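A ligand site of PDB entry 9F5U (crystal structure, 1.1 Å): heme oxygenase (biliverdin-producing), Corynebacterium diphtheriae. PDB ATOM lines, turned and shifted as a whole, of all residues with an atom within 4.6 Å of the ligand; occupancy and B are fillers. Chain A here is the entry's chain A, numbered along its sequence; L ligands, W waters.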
ATOM      1  N   ALA A   9       7.828 -18.059 -25.986  1.00  0.00           N
ATOM      2  CA  ALA A   9       6.364 -18.123 -26.088  1.00  0.00           C
ATOM      3  C   ALA A   9       5.928 -18.520 -27.484  1.00  0.00           C
ATOM      4  O   ALA A   9       5.016 -19.340 -27.656  1.00  0.00           O
ATOM      5  CB  ALA A   9       5.732 -16.799 -25.657  1.00  0.00           C
ATOM      6  N   LYS A  13       4.058 -22.071 -28.708  1.00  0.00           N
ATOM      7  CA  LYS A  13       2.829 -22.074 -29.485  1.00  0.00           C
ATOM      8  C   LYS A  13       2.989 -22.873 -30.771  1.00  0.00           C
ATOM      9  O   LYS A  13       2.147 -23.722 -31.109  1.00  0.00           O
ATOM     10  CB  LYS A  13       2.400 -20.642 -29.790  1.00  0.00           C
ATOM     11  CG  LYS A  13       1.098 -20.531 -30.562  1.00  0.00           C
ATOM     12  CD  LYS A  13       0.650 -19.081 -30.647  1.00  0.00           C
ATOM     13  CE  LYS A  13      -0.606 -18.920 -31.475  1.00  0.00           C
ATOM     14  NZ  LYS A  13      -1.115 -17.528 -31.408  1.00  0.00           N
ATOM     15  N   HIS A  20      -2.582 -29.049 -30.319  1.00  0.00           N
ATOM     16  CA  HIS A  20      -3.774 -28.318 -29.926  1.00  0.00           C
ATOM     17  C   HIS A  20      -4.937 -28.634 -30.854  1.00  0.00           C
ATOM     18  O   HIS A  20      -6.070 -28.865 -30.408  1.00  0.00           O
ATOM     19  CB  HIS A  20      -3.511 -26.825 -29.907  1.00  0.00           C
ATOM     20  CG  HIS A  20      -4.600 -26.075 -29.237  1.00  0.00           C
ATOM     21  ND1 HIS A  20      -5.725 -25.631 -29.912  1.00  0.00           N
ATOM     22  CD2 HIS A  20      -4.782 -25.753 -27.938  1.00  0.00           C
ATOM     23  CE1 HIS A  20      -6.526 -25.033 -29.050  1.00  0.00           C
ATOM     24  NE2 HIS A  20      -5.970 -25.089 -27.859  1.00  0.00           N
ATOM     25  N   ALA A  23      -6.272 -31.993 -30.104  1.00  0.00           N
ATOM     26  CA  ALA A  23      -7.083 -31.988 -28.889  1.00  0.00           C
ATOM     27  C   ALA A  23      -8.500 -31.538 -29.172  1.00  0.00           C
ATOM     28  O   ALA A  23      -9.465 -32.124 -28.658  1.00  0.00           O
ATOM     29  CB  ALA A  23      -6.433 -31.080 -27.845  1.00  0.00           C
ATOM     30  N   GLU A  24      -8.664 -30.481 -29.971  1.00  0.00           N
ATOM     31  CA  GLU A  24     -10.005 -30.014 -30.311  1.00  0.00           C
ATOM     32  C   GLU A  24     -10.805 -31.070 -31.057  1.00  0.00           C
ATOM     33  O   GLU A  24     -12.039 -31.085 -31.002  1.00  0.00           O
ATOM     34  CB  GLU A  24      -9.926 -28.736 -31.153  1.00  0.00           C
ATOM     35  CG  GLU A  24      -9.457 -27.513 -30.382  1.00  0.00           C
ATOM     36  CD  GLU A  24      -9.379 -26.265 -31.246  1.00  0.00           C
ATOM     37  OE1 GLU A  24      -9.468 -26.381 -32.483  1.00  0.00           O
ATOM     38  OE2 GLU A  24      -9.224 -25.166 -30.687  1.00  0.00           O
ATOM     39  N   MET A  29     -13.844 -34.906 -26.503  1.00  0.00           N
ATOM     40  CA  MET A  29     -13.985 -33.486 -26.273  1.00  0.00           C
ATOM     41  C   MET A  29     -14.862 -32.844 -27.346  1.00  0.00           C
ATOM     42  O   MET A  29     -15.674 -31.961 -27.053  1.00  0.00           O
ATOM     43  CB  MET A  29     -12.623 -32.821 -26.190  1.00  0.00           C
ATOM     44  CG  MET A  29     -12.640 -31.457 -25.516  1.00  0.00           C
ATOM     45  SD  MET A  29     -13.228 -31.561 -23.813  1.00  0.00           S
ATOM     46  CE  MET A  29     -12.930 -29.883 -23.310  1.00  0.00           C
ATOM     47  N   LEU A  33     -18.202 -30.731 -26.566  1.00  0.00           N
ATOM     48  CA  LEU A  33     -18.352 -29.334 -26.972  1.00  0.00           C
ATOM     49  C   LEU A  33     -19.491 -29.117 -27.949  1.00  0.00           C
ATOM     50  O   LEU A  33     -20.071 -28.029 -27.976  1.00  0.00           O
ATOM     51  CB  LEU A  33     -17.056 -28.827 -27.590  1.00  0.00           C
ATOM     52  CG  LEU A  33     -15.859 -28.855 -26.663  1.00  0.00           C
ATOM     53  CD1 LEU A  33     -14.655 -28.230 -27.324  1.00  0.00           C
ATOM     54  CD2 LEU A  33     -16.194 -28.158 -25.338  1.00  0.00           C
ATOM     55  N   TYR A 130       2.414 -23.591 -18.638  1.00  0.00           N
ATOM     56  CA  TYR A 130       1.967 -23.026 -19.910  1.00  0.00           C
ATOM     57  C   TYR A 130       0.798 -23.832 -20.481  1.00  0.00           C
ATOM     58  O   TYR A 130      -0.242 -23.269 -20.833  1.00  0.00           O
ATOM     59  CB  TYR A 130       3.156 -23.024 -20.882  1.00  0.00           C
ATOM     60  CG  TYR A 130       2.757 -22.887 -22.332  1.00  0.00           C
ATOM     61  CD1 TYR A 130       2.482 -21.645 -22.876  1.00  0.00           C
ATOM     62  CD2 TYR A 130       2.666 -23.998 -23.150  1.00  0.00           C
ATOM     63  CE1 TYR A 130       2.103 -21.510 -24.197  1.00  0.00           C
ATOM     64  CE2 TYR A 130       2.281 -23.886 -24.466  1.00  0.00           C
ATOM     65  CZ  TYR A 130       2.005 -22.640 -24.997  1.00  0.00           C
ATOM     66  OH  TYR A 130       1.610 -22.548 -26.318  1.00  0.00           O
ATOM     67  N   VAL A 131       0.962 -25.150 -20.576  1.00  0.00           N
ATOM     68  CA  VAL A 131      -0.028 -25.984 -21.251  1.00  0.00           C
ATOM     69  C   VAL A 131      -1.375 -25.881 -20.565  1.00  0.00           C
ATOM     70  O   VAL A 131      -2.403 -25.775 -21.240  1.00  0.00           O
ATOM     71  CB  VAL A 131       0.486 -27.430 -21.363  1.00  0.00           C
ATOM     72  CG1 VAL A 131      -0.641 -28.368 -21.807  1.00  0.00           C
ATOM     73  CG2 VAL A 131       1.654 -27.494 -22.330  1.00  0.00           C
ATOM     74  N   ARG A 132      -1.408 -25.925 -19.228  1.00  0.00           N
ATOM     75  CA  ARG A 132      -2.684 -25.796 -18.537  1.00  0.00           C
ATOM     76  C   ARG A 132      -3.134 -24.348 -18.415  1.00  0.00           C
ATOM     77  O   ARG A 132      -4.208 -23.983 -18.924  1.00  0.00           O
ATOM     78  CB  ARG A 132      -2.678 -26.507 -17.184  1.00  0.00           C
ATOM     79  CG  ARG A 132      -2.769 -28.048 -17.267  1.00  0.00           C
ATOM     80  CD  ARG A 132      -3.828 -28.592 -18.235  1.00  0.00           C
ATOM     81  NE  ARG A 132      -5.124 -27.967 -18.083  1.00  0.00           N
ATOM     82  CZ  ARG A 132      -6.171 -28.196 -18.874  1.00  0.00           C
ATOM     83  NH1 ARG A 132      -6.130 -29.157 -19.787  1.00  0.00           N
ATOM     84  NH2 ARG A 132      -7.258 -27.447 -18.755  1.00  0.00           N
ATOM     85  N   LEU A 134      -2.049 -21.220 -19.467  1.00  0.00           N
ATOM     86  CA  LEU A 134      -2.240 -20.333 -20.598  1.00  0.00           C
ATOM     87  C   LEU A 134      -3.397 -20.819 -21.470  1.00  0.00           C
ATOM     88  O   LEU A 134      -4.133 -19.991 -22.020  1.00  0.00           O
ATOM     89  CB  LEU A 134      -0.961 -20.090 -21.407  1.00  0.00           C
ATOM     90  CG  LEU A 134      -1.095 -18.895 -22.380  1.00  0.00           C
ATOM     91  CD1 LEU A 134      -1.473 -17.588 -21.655  1.00  0.00           C
ATOM     92  CD2 LEU A 134       0.176 -18.719 -23.189  1.00  0.00           C
ATOM     93  N   GLY A 135      -3.585 -22.130 -21.573  1.00  0.00           N
ATOM     94  CA  GLY A 135      -4.768 -22.638 -22.260  1.00  0.00           C
ATOM     95  C   GLY A 135      -6.053 -22.256 -21.556  1.00  0.00           C
ATOM     96  O   GLY A 135      -7.042 -21.903 -22.195  1.00  0.00           O
ATOM     97  N   SER A 138      -6.635 -18.549 -22.123  1.00  0.00           N
ATOM     98  CA  SER A 138      -6.855 -18.205 -23.527  1.00  0.00           C
ATOM     99  C   SER A 138      -8.140 -18.786 -24.088  1.00  0.00           C
ATOM    100  O   SER A 138      -8.792 -18.146 -24.918  1.00  0.00           O
ATOM    101  CB  SER A 138      -5.675 -18.687 -24.378  1.00  0.00           C
ATOM    102  OG  SER A 138      -4.460 -18.093 -23.956  1.00  0.00           O
ATOM    103  N   GLY A 139      -8.509 -20.000 -23.669  1.00  0.00           N
ATOM    104  CA  GLY A 139      -9.644 -20.693 -24.253  1.00  0.00           C
ATOM    105  C   GLY A 139     -10.743 -21.073 -23.295  1.00  0.00           C
ATOM    106  O   GLY A 139     -11.788 -21.572 -23.712  1.00  0.00           O
ATOM    107  N   VAL A 142     -14.395 -19.984 -23.911  1.00  0.00           N
ATOM    108  CA  VAL A 142     -15.092 -20.674 -24.999  1.00  0.00           C
ATOM    109  C   VAL A 142     -15.698 -21.975 -24.487  1.00  0.00           C
ATOM    110  O   VAL A 142     -16.856 -22.292 -24.752  1.00  0.00           O
ATOM    111  CB  VAL A 142     -14.118 -20.908 -26.163  1.00  0.00           C
ATOM    112  CG1 VAL A 142     -14.734 -21.869 -27.196  1.00  0.00           C
ATOM    113  CG2 VAL A 142     -13.714 -19.596 -26.821  1.00  0.00           C
ATOM    114  N   ILE A 143     -14.904 -22.753 -23.756  1.00  0.00           N
ATOM    115  CA  ILE A 143     -15.373 -24.029 -23.242  1.00  0.00           C
ATOM    116  C   ILE A 143     -16.544 -23.825 -22.287  1.00  0.00           C
ATOM    117  O   ILE A 143     -17.576 -24.504 -22.380  1.00  0.00           O
ATOM    118  CB  ILE A 143     -14.218 -24.814 -22.599  1.00  0.00           C
ATOM    119  CG1 ILE A 143     -13.145 -25.140 -23.644  1.00  0.00           C
ATOM    120  CG2 ILE A 143     -14.738 -26.084 -21.925  1.00  0.00           C
ATOM    121  CD1 ILE A 143     -11.839 -25.659 -23.047  1.00  0.00           C
ATOM    122  N   MET A 146     -19.781 -23.073 -24.036  1.00  0.00           N
ATOM    123  CA  MET A 146     -20.418 -24.218 -24.676  1.00  0.00           C
ATOM    124  C   MET A 146     -21.121 -25.124 -23.670  1.00  0.00           C
ATOM    125  O   MET A 146     -22.148 -25.731 -24.000  1.00  0.00           O
ATOM    126  CB  MET A 146     -19.395 -24.993 -25.512  1.00  0.00           C
ATOM    127  CG  MET A 146     -18.910 -24.196 -26.705  1.00  0.00           C
ATOM    128  SD  MET A 146     -17.976 -25.233 -27.817  1.00  0.00           S
ATOM    129  CE  MET A 146     -16.688 -24.104 -28.334  1.00  0.00           C
ATOM    130  N   ARG A 177       3.202 -14.239 -21.661  1.00  0.00           N
ATOM    131  CA  ARG A 177       4.066 -14.618 -22.771  1.00  0.00           C
ATOM    132  C   ARG A 177       5.427 -13.919 -22.674  1.00  0.00           C
ATOM    133  O   ARG A 177       6.462 -14.512 -22.985  1.00  0.00           O
ATOM    134  CB  ARG A 177       3.387 -14.322 -24.105  1.00  0.00           C
ATOM    135  CG  ARG A 177       2.193 -15.235 -24.352  1.00  0.00           C
ATOM    136  CD  ARG A 177       1.641 -15.120 -25.763  1.00  0.00           C
ATOM    137  NE  ARG A 177       0.430 -15.917 -25.923  1.00  0.00           N
ATOM    138  CZ  ARG A 177      -0.803 -15.443 -25.799  1.00  0.00           C
ATOM    139  NH1 ARG A 177      -1.027 -14.156 -25.566  1.00  0.00           N
ATOM    140  NH2 ARG A 177      -1.834 -16.276 -25.907  1.00  0.00           N
ATOM    141  N   PHE A 201       0.808 -32.032 -23.501  1.00  0.00           N
ATOM    142  CA  PHE A 201      -0.319 -32.175 -24.421  1.00  0.00           C
ATOM    143  C   PHE A 201      -0.708 -33.639 -24.585  1.00  0.00           C
ATOM    144  O   PHE A 201      -1.910 -33.954 -24.615  1.00  0.00           O
ATOM    145  CB  PHE A 201      -0.042 -31.515 -25.768  1.00  0.00           C
ATOM    146  CG  PHE A 201      -0.578 -30.117 -25.884  1.00  0.00           C
ATOM    147  CD1 PHE A 201      -1.887 -29.873 -26.291  1.00  0.00           C
ATOM    148  CD2 PHE A 201       0.237 -29.027 -25.577  1.00  0.00           C
ATOM    149  CE1 PHE A 201      -2.364 -28.572 -26.389  1.00  0.00           C
ATOM    150  CE2 PHE A 201      -0.235 -27.733 -25.702  1.00  0.00           C
ATOM    151  CZ  PHE A 201      -1.545 -27.502 -26.092  1.00  0.00           C
ATOM    152  N   ASN A 204      -2.745 -34.754 -21.625  1.00  0.00           N
ATOM    153  CA  ASN A 204      -4.077 -34.174 -21.638  1.00  0.00           C
ATOM    154  C   ASN A 204      -4.960 -34.846 -22.679  1.00  0.00           C
ATOM    155  O   ASN A 204      -6.153 -35.080 -22.440  1.00  0.00           O
ATOM    156  CB  ASN A 204      -3.994 -32.653 -21.845  1.00  0.00           C
ATOM    157  CG  ASN A 204      -3.760 -31.939 -20.542  1.00  0.00           C
ATOM    158  OD1 ASN A 204      -4.706 -31.685 -19.805  1.00  0.00           O
ATOM    159  ND2 ASN A 204      -2.498 -31.618 -20.224  1.00  0.00           N
ATOM    160  N   HIS A 205      -4.378 -35.208 -23.831  1.00  0.00           N
ATOM    161  CA  HIS A 205      -5.141 -35.925 -24.836  1.00  0.00           C
ATOM    162  C   HIS A 205      -5.564 -37.299 -24.321  1.00  0.00           C
ATOM    163  O   HIS A 205      -6.702 -37.742 -24.553  1.00  0.00           O
ATOM    164  CB  HIS A 205      -4.294 -36.019 -26.112  1.00  0.00           C
ATOM    165  CG  HIS A 205      -5.094 -36.310 -27.333  1.00  0.00           C
ATOM    166  ND1 HIS A 205      -4.954 -35.589 -28.511  1.00  0.00           N
ATOM    167  CD2 HIS A 205      -6.044 -37.242 -27.581  1.00  0.00           C
ATOM    168  CE1 HIS A 205      -5.783 -36.073 -29.420  1.00  0.00           C
ATOM    169  NE2 HIS A 205      -6.452 -37.074 -28.878  1.00  0.00           N
ATOM    170  N   PHE A 208      -8.674 -37.338 -22.207  1.00  0.00           N
ATOM    171  CA  PHE A 208      -9.894 -37.368 -22.999  1.00  0.00           C
ATOM    172  C   PHE A 208     -10.175 -38.776 -23.505  1.00  0.00           C
ATOM    173  O   PHE A 208     -11.332 -39.219 -23.534  1.00  0.00           O
ATOM    174  CB  PHE A 208      -9.775 -36.444 -24.213  1.00  0.00           C
ATOM    175  CG  PHE A 208      -9.609 -34.989 -23.884  1.00  0.00           C
ATOM    176  CD1 PHE A 208     -10.098 -34.428 -22.713  1.00  0.00           C
ATOM    177  CD2 PHE A 208      -8.975 -34.167 -24.793  1.00  0.00           C
ATOM    178  CE1 PHE A 208      -9.936 -33.080 -22.447  1.00  0.00           C
ATOM    179  CE2 PHE A 208      -8.810 -32.822 -24.541  1.00  0.00           C
ATOM    180  CZ  PHE A 208      -9.290 -32.271 -23.366  1.00  0.00           C
HETATM  181 CO1  LIG L   1      -6.767 -24.501 -25.971  1.00  0.00          CO
HETATM  182  C1  LIG L   1      -5.267 -21.559 -26.699  1.00  0.00           C
HETATM  183  C2  LIG L   1      -4.020 -25.514 -24.224  1.00  0.00           C
HETATM  184  C3  LIG L   1      -8.056 -27.641 -25.817  1.00  0.00           C
HETATM  185  C4  LIG L   1      -9.771 -23.299 -27.083  1.00  0.00           C
HETATM  186  N1  LIG L   1      -5.042 -23.717 -25.571  1.00  0.00           N
HETATM  187  C5  LIG L   1      -4.534 -22.523 -25.927  1.00  0.00           C
HETATM  188  C6  LIG L   1      -3.171 -22.234 -25.490  1.00  0.00           C
HETATM  189  C7  LIG L   1      -2.808 -23.416 -24.762  1.00  0.00           C
HETATM  190  C8  LIG L   1      -4.010 -24.237 -24.878  1.00  0.00           C
HETATM  191  C9  LIG L   1      -1.539 -23.736 -24.048  1.00  0.00           C
HETATM  192  C10 LIG L   1      -2.342 -21.005 -25.706  1.00  0.00           C
HETATM  193  C11 LIG L   1      -1.552 -21.112 -27.011  1.00  0.00           C
HETATM  194  C12 LIG L   1      -0.568 -19.960 -27.067  1.00  0.00           C
HETATM  195  O1  LIG L   1      -1.023 -18.809 -27.221  1.00  0.00           O
HETATM  196  O2  LIG L   1       0.653 -20.193 -26.919  1.00  0.00           O
HETATM  197  N2  LIG L   1      -6.199 -26.174 -25.175  1.00  0.00           N
HETATM  198  C13 LIG L   1      -5.068 -26.472 -24.467  1.00  0.00           C
HETATM  199  C14 LIG L   1      -4.909 -27.842 -23.962  1.00  0.00           C
HETATM  200  C15 LIG L   1      -6.117 -28.449 -24.461  1.00  0.00           C
HETATM  201  C16 LIG L   1      -6.805 -27.380 -25.163  1.00  0.00           C
HETATM  202  C17 LIG L   1      -3.811 -28.448 -23.157  1.00  0.00           C
HETATM  203  C18 LIG L   1      -6.587 -29.848 -24.293  1.00  0.00           C
HETATM  204  C19 LIG L   1      -5.765 -30.882 -24.328  1.00  0.00           C
HETATM  205  N3  LIG L   1      -8.488 -25.276 -26.380  1.00  0.00           N
HETATM  206  C20 LIG L   1      -8.886 -26.565 -26.300  1.00  0.00           C
HETATM  207  C21 LIG L   1     -10.258 -26.901 -26.684  1.00  0.00           C
HETATM  208  C22 LIG L   1     -10.740 -25.594 -27.063  1.00  0.00           C
HETATM  209  C23 LIG L   1      -9.613 -24.697 -26.830  1.00  0.00           C
HETATM  210  C24 LIG L   1     -10.933 -28.243 -26.687  1.00  0.00           C
HETATM  211  C25 LIG L   1     -12.084 -25.209 -27.561  1.00  0.00           C
HETATM  212  C26 LIG L   1     -12.687 -25.966 -28.449  1.00  0.00           C
HETATM  213  N4  LIG L   1      -7.378 -22.823 -26.702  1.00  0.00           N
HETATM  214  C27 LIG L   1      -8.622 -22.440 -27.103  1.00  0.00           C
HETATM  215  C28 LIG L   1      -8.796 -21.082 -27.606  1.00  0.00           C
HETATM  216  C29 LIG L   1      -7.456 -20.557 -27.501  1.00  0.00           C
HETATM  217  C30 LIG L   1      -6.687 -21.695 -26.939  1.00  0.00           C
HETATM  218  C31 LIG L   1     -10.039 -20.402 -28.107  1.00  0.00           C
HETATM  219  C32 LIG L   1      -6.974 -19.198 -27.885  1.00  0.00           C
HETATM  220  C33 LIG L   1      -6.437 -19.280 -29.309  1.00  0.00           C
HETATM  221  C34 LIG L   1      -7.474 -19.788 -30.282  1.00  0.00           C
HETATM  222  O3  LIG L   1      -7.208 -20.797 -30.972  1.00  0.00           O
HETATM  223  O4  LIG L   1      -8.554 -19.180 -30.372  1.00  0.00           O
HETATM  224  O   HOH W   1     -10.647 -20.730 -31.355  1.00  0.00           O
HETATM  225  O   HOH W   2      -6.034 -21.146 -33.429  1.00  0.00           O
HETATM  226  O   HOH W   3       2.500 -18.227 -26.831  1.00  0.00           O
HETATM  227  O   HOH W   4      -8.644 -22.780 -32.534  1.00  0.00           O
HETATM  228  O   HOH W   5      -7.548 -23.956 -24.232  1.00  0.00           O
HETATM  229  O   HOH W   6      -4.020 -32.677 -25.969  1.00  0.00           O
HETATM  230  O   HOH W   7      -8.437 -28.487 -21.912  1.00  0.00           O
HETATM  231  O   HOH W   8      -7.713 -25.761 -22.272  1.00  0.00           O
HETATM  232  O   HOH W   9      -3.471 -18.500 -28.048  1.00  0.00           O
HETATM  233  O   HOH W  10      -0.757 -16.320 -29.018  1.00  0.00           O
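The side-chain hydroxyl (OG) of Ser 138 lies within hydrogen-bond range of the backbone carbonyl oxygen (O) of Leu 134 (2.7 Å).
OH of Tyr 130 lies close to N of Lys 13, at 3.5 Å.
The guanidinium group of Arg 132 sits at hydrogen-bond distance from the side-chain amide oxygen of Asn 204.
OH of Tyr 130 lies within hydrogen-bond range of O2 of the ligand (2.6 Å).
The guanidinium group of Arg 177 is in salt-bridge range of an oxygen (O1) of the ligand, at 3.0 Å.
A cobalt atom (CO1) of the ligand is bound by a ring nitrogen (NE2) of His 20, at 2.1 Å.
Water W9 lies within hydrogen-bond range of an oxygen (O1) of the ligand and the guanidinium group of Arg 177.
Water W3 lies within hydrogen-bond range of an oxygen (O2) of the ligand (2.7 Å), the backbone carbonyl oxygen (O) of Ala 9 (2.9 Å) and the guanidinium group (NE) of Arg 177 (3.2 Å).
Water W4 lies within hydrogen-bond range of O3 of the ligand (2.9 Å) and OE2 of Glu 24 (3.1 Å).
Water W10 lies within hydrogen-bond range of the side-chain amino group (NZ) of Lys 13 (2.7 Å), an oxygen (O1) of the ligand (3.1 Å) and the guanidinium group (NH2) of Arg 177 (3.3 Å).
Lys 13 touches the ligand.
Ala 23 touches the ligand.
Glu 24 touches the ligand.
Met 29 touches the ligand (CG to C24, 3.8 Å).
Leu 33 touches the ligand.
O of Val 131 touches C2 of the ligand, at 3.4 Å.
Gly 135 touches the ligand (CA to C8, 3.2 Å).
Ser 138 touches the ligand (O to C32, 3.6 Å).
Gly 139 touches the ligand (CA to C28, 3.5 Å).
Val 142 touches the ligand (CG2 to C31, 3.98 Å).
Phe 201 touches the ligand (CE1 to C17, 3.5 Å).
CB of Asn 204 touches C19 of the ligand, 3.5 Å away.
Phe 208 touches the ligand (CE2 to C19, 3.6 Å).
Hydrophobic or aromatic side chains that line the ligand: His 20, Ala 23, Met 29, Leu 33, Tyr 130, Val 131, Val 142, Phe 201 and Phe 208.
16 residues have an atom within 4 Å of the ligand: Lys 13, His 20, Ala 23, Glu 24, Met 29, Leu 33, Tyr 130, Val 131, Gly 135, Ser 138, Gly 139, Val 142, Arg 177, Phe 201, Asn 204 and Phe 208.
The nearest printed residue that does not touch the ligand is Leu 134 (4.04 Å).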
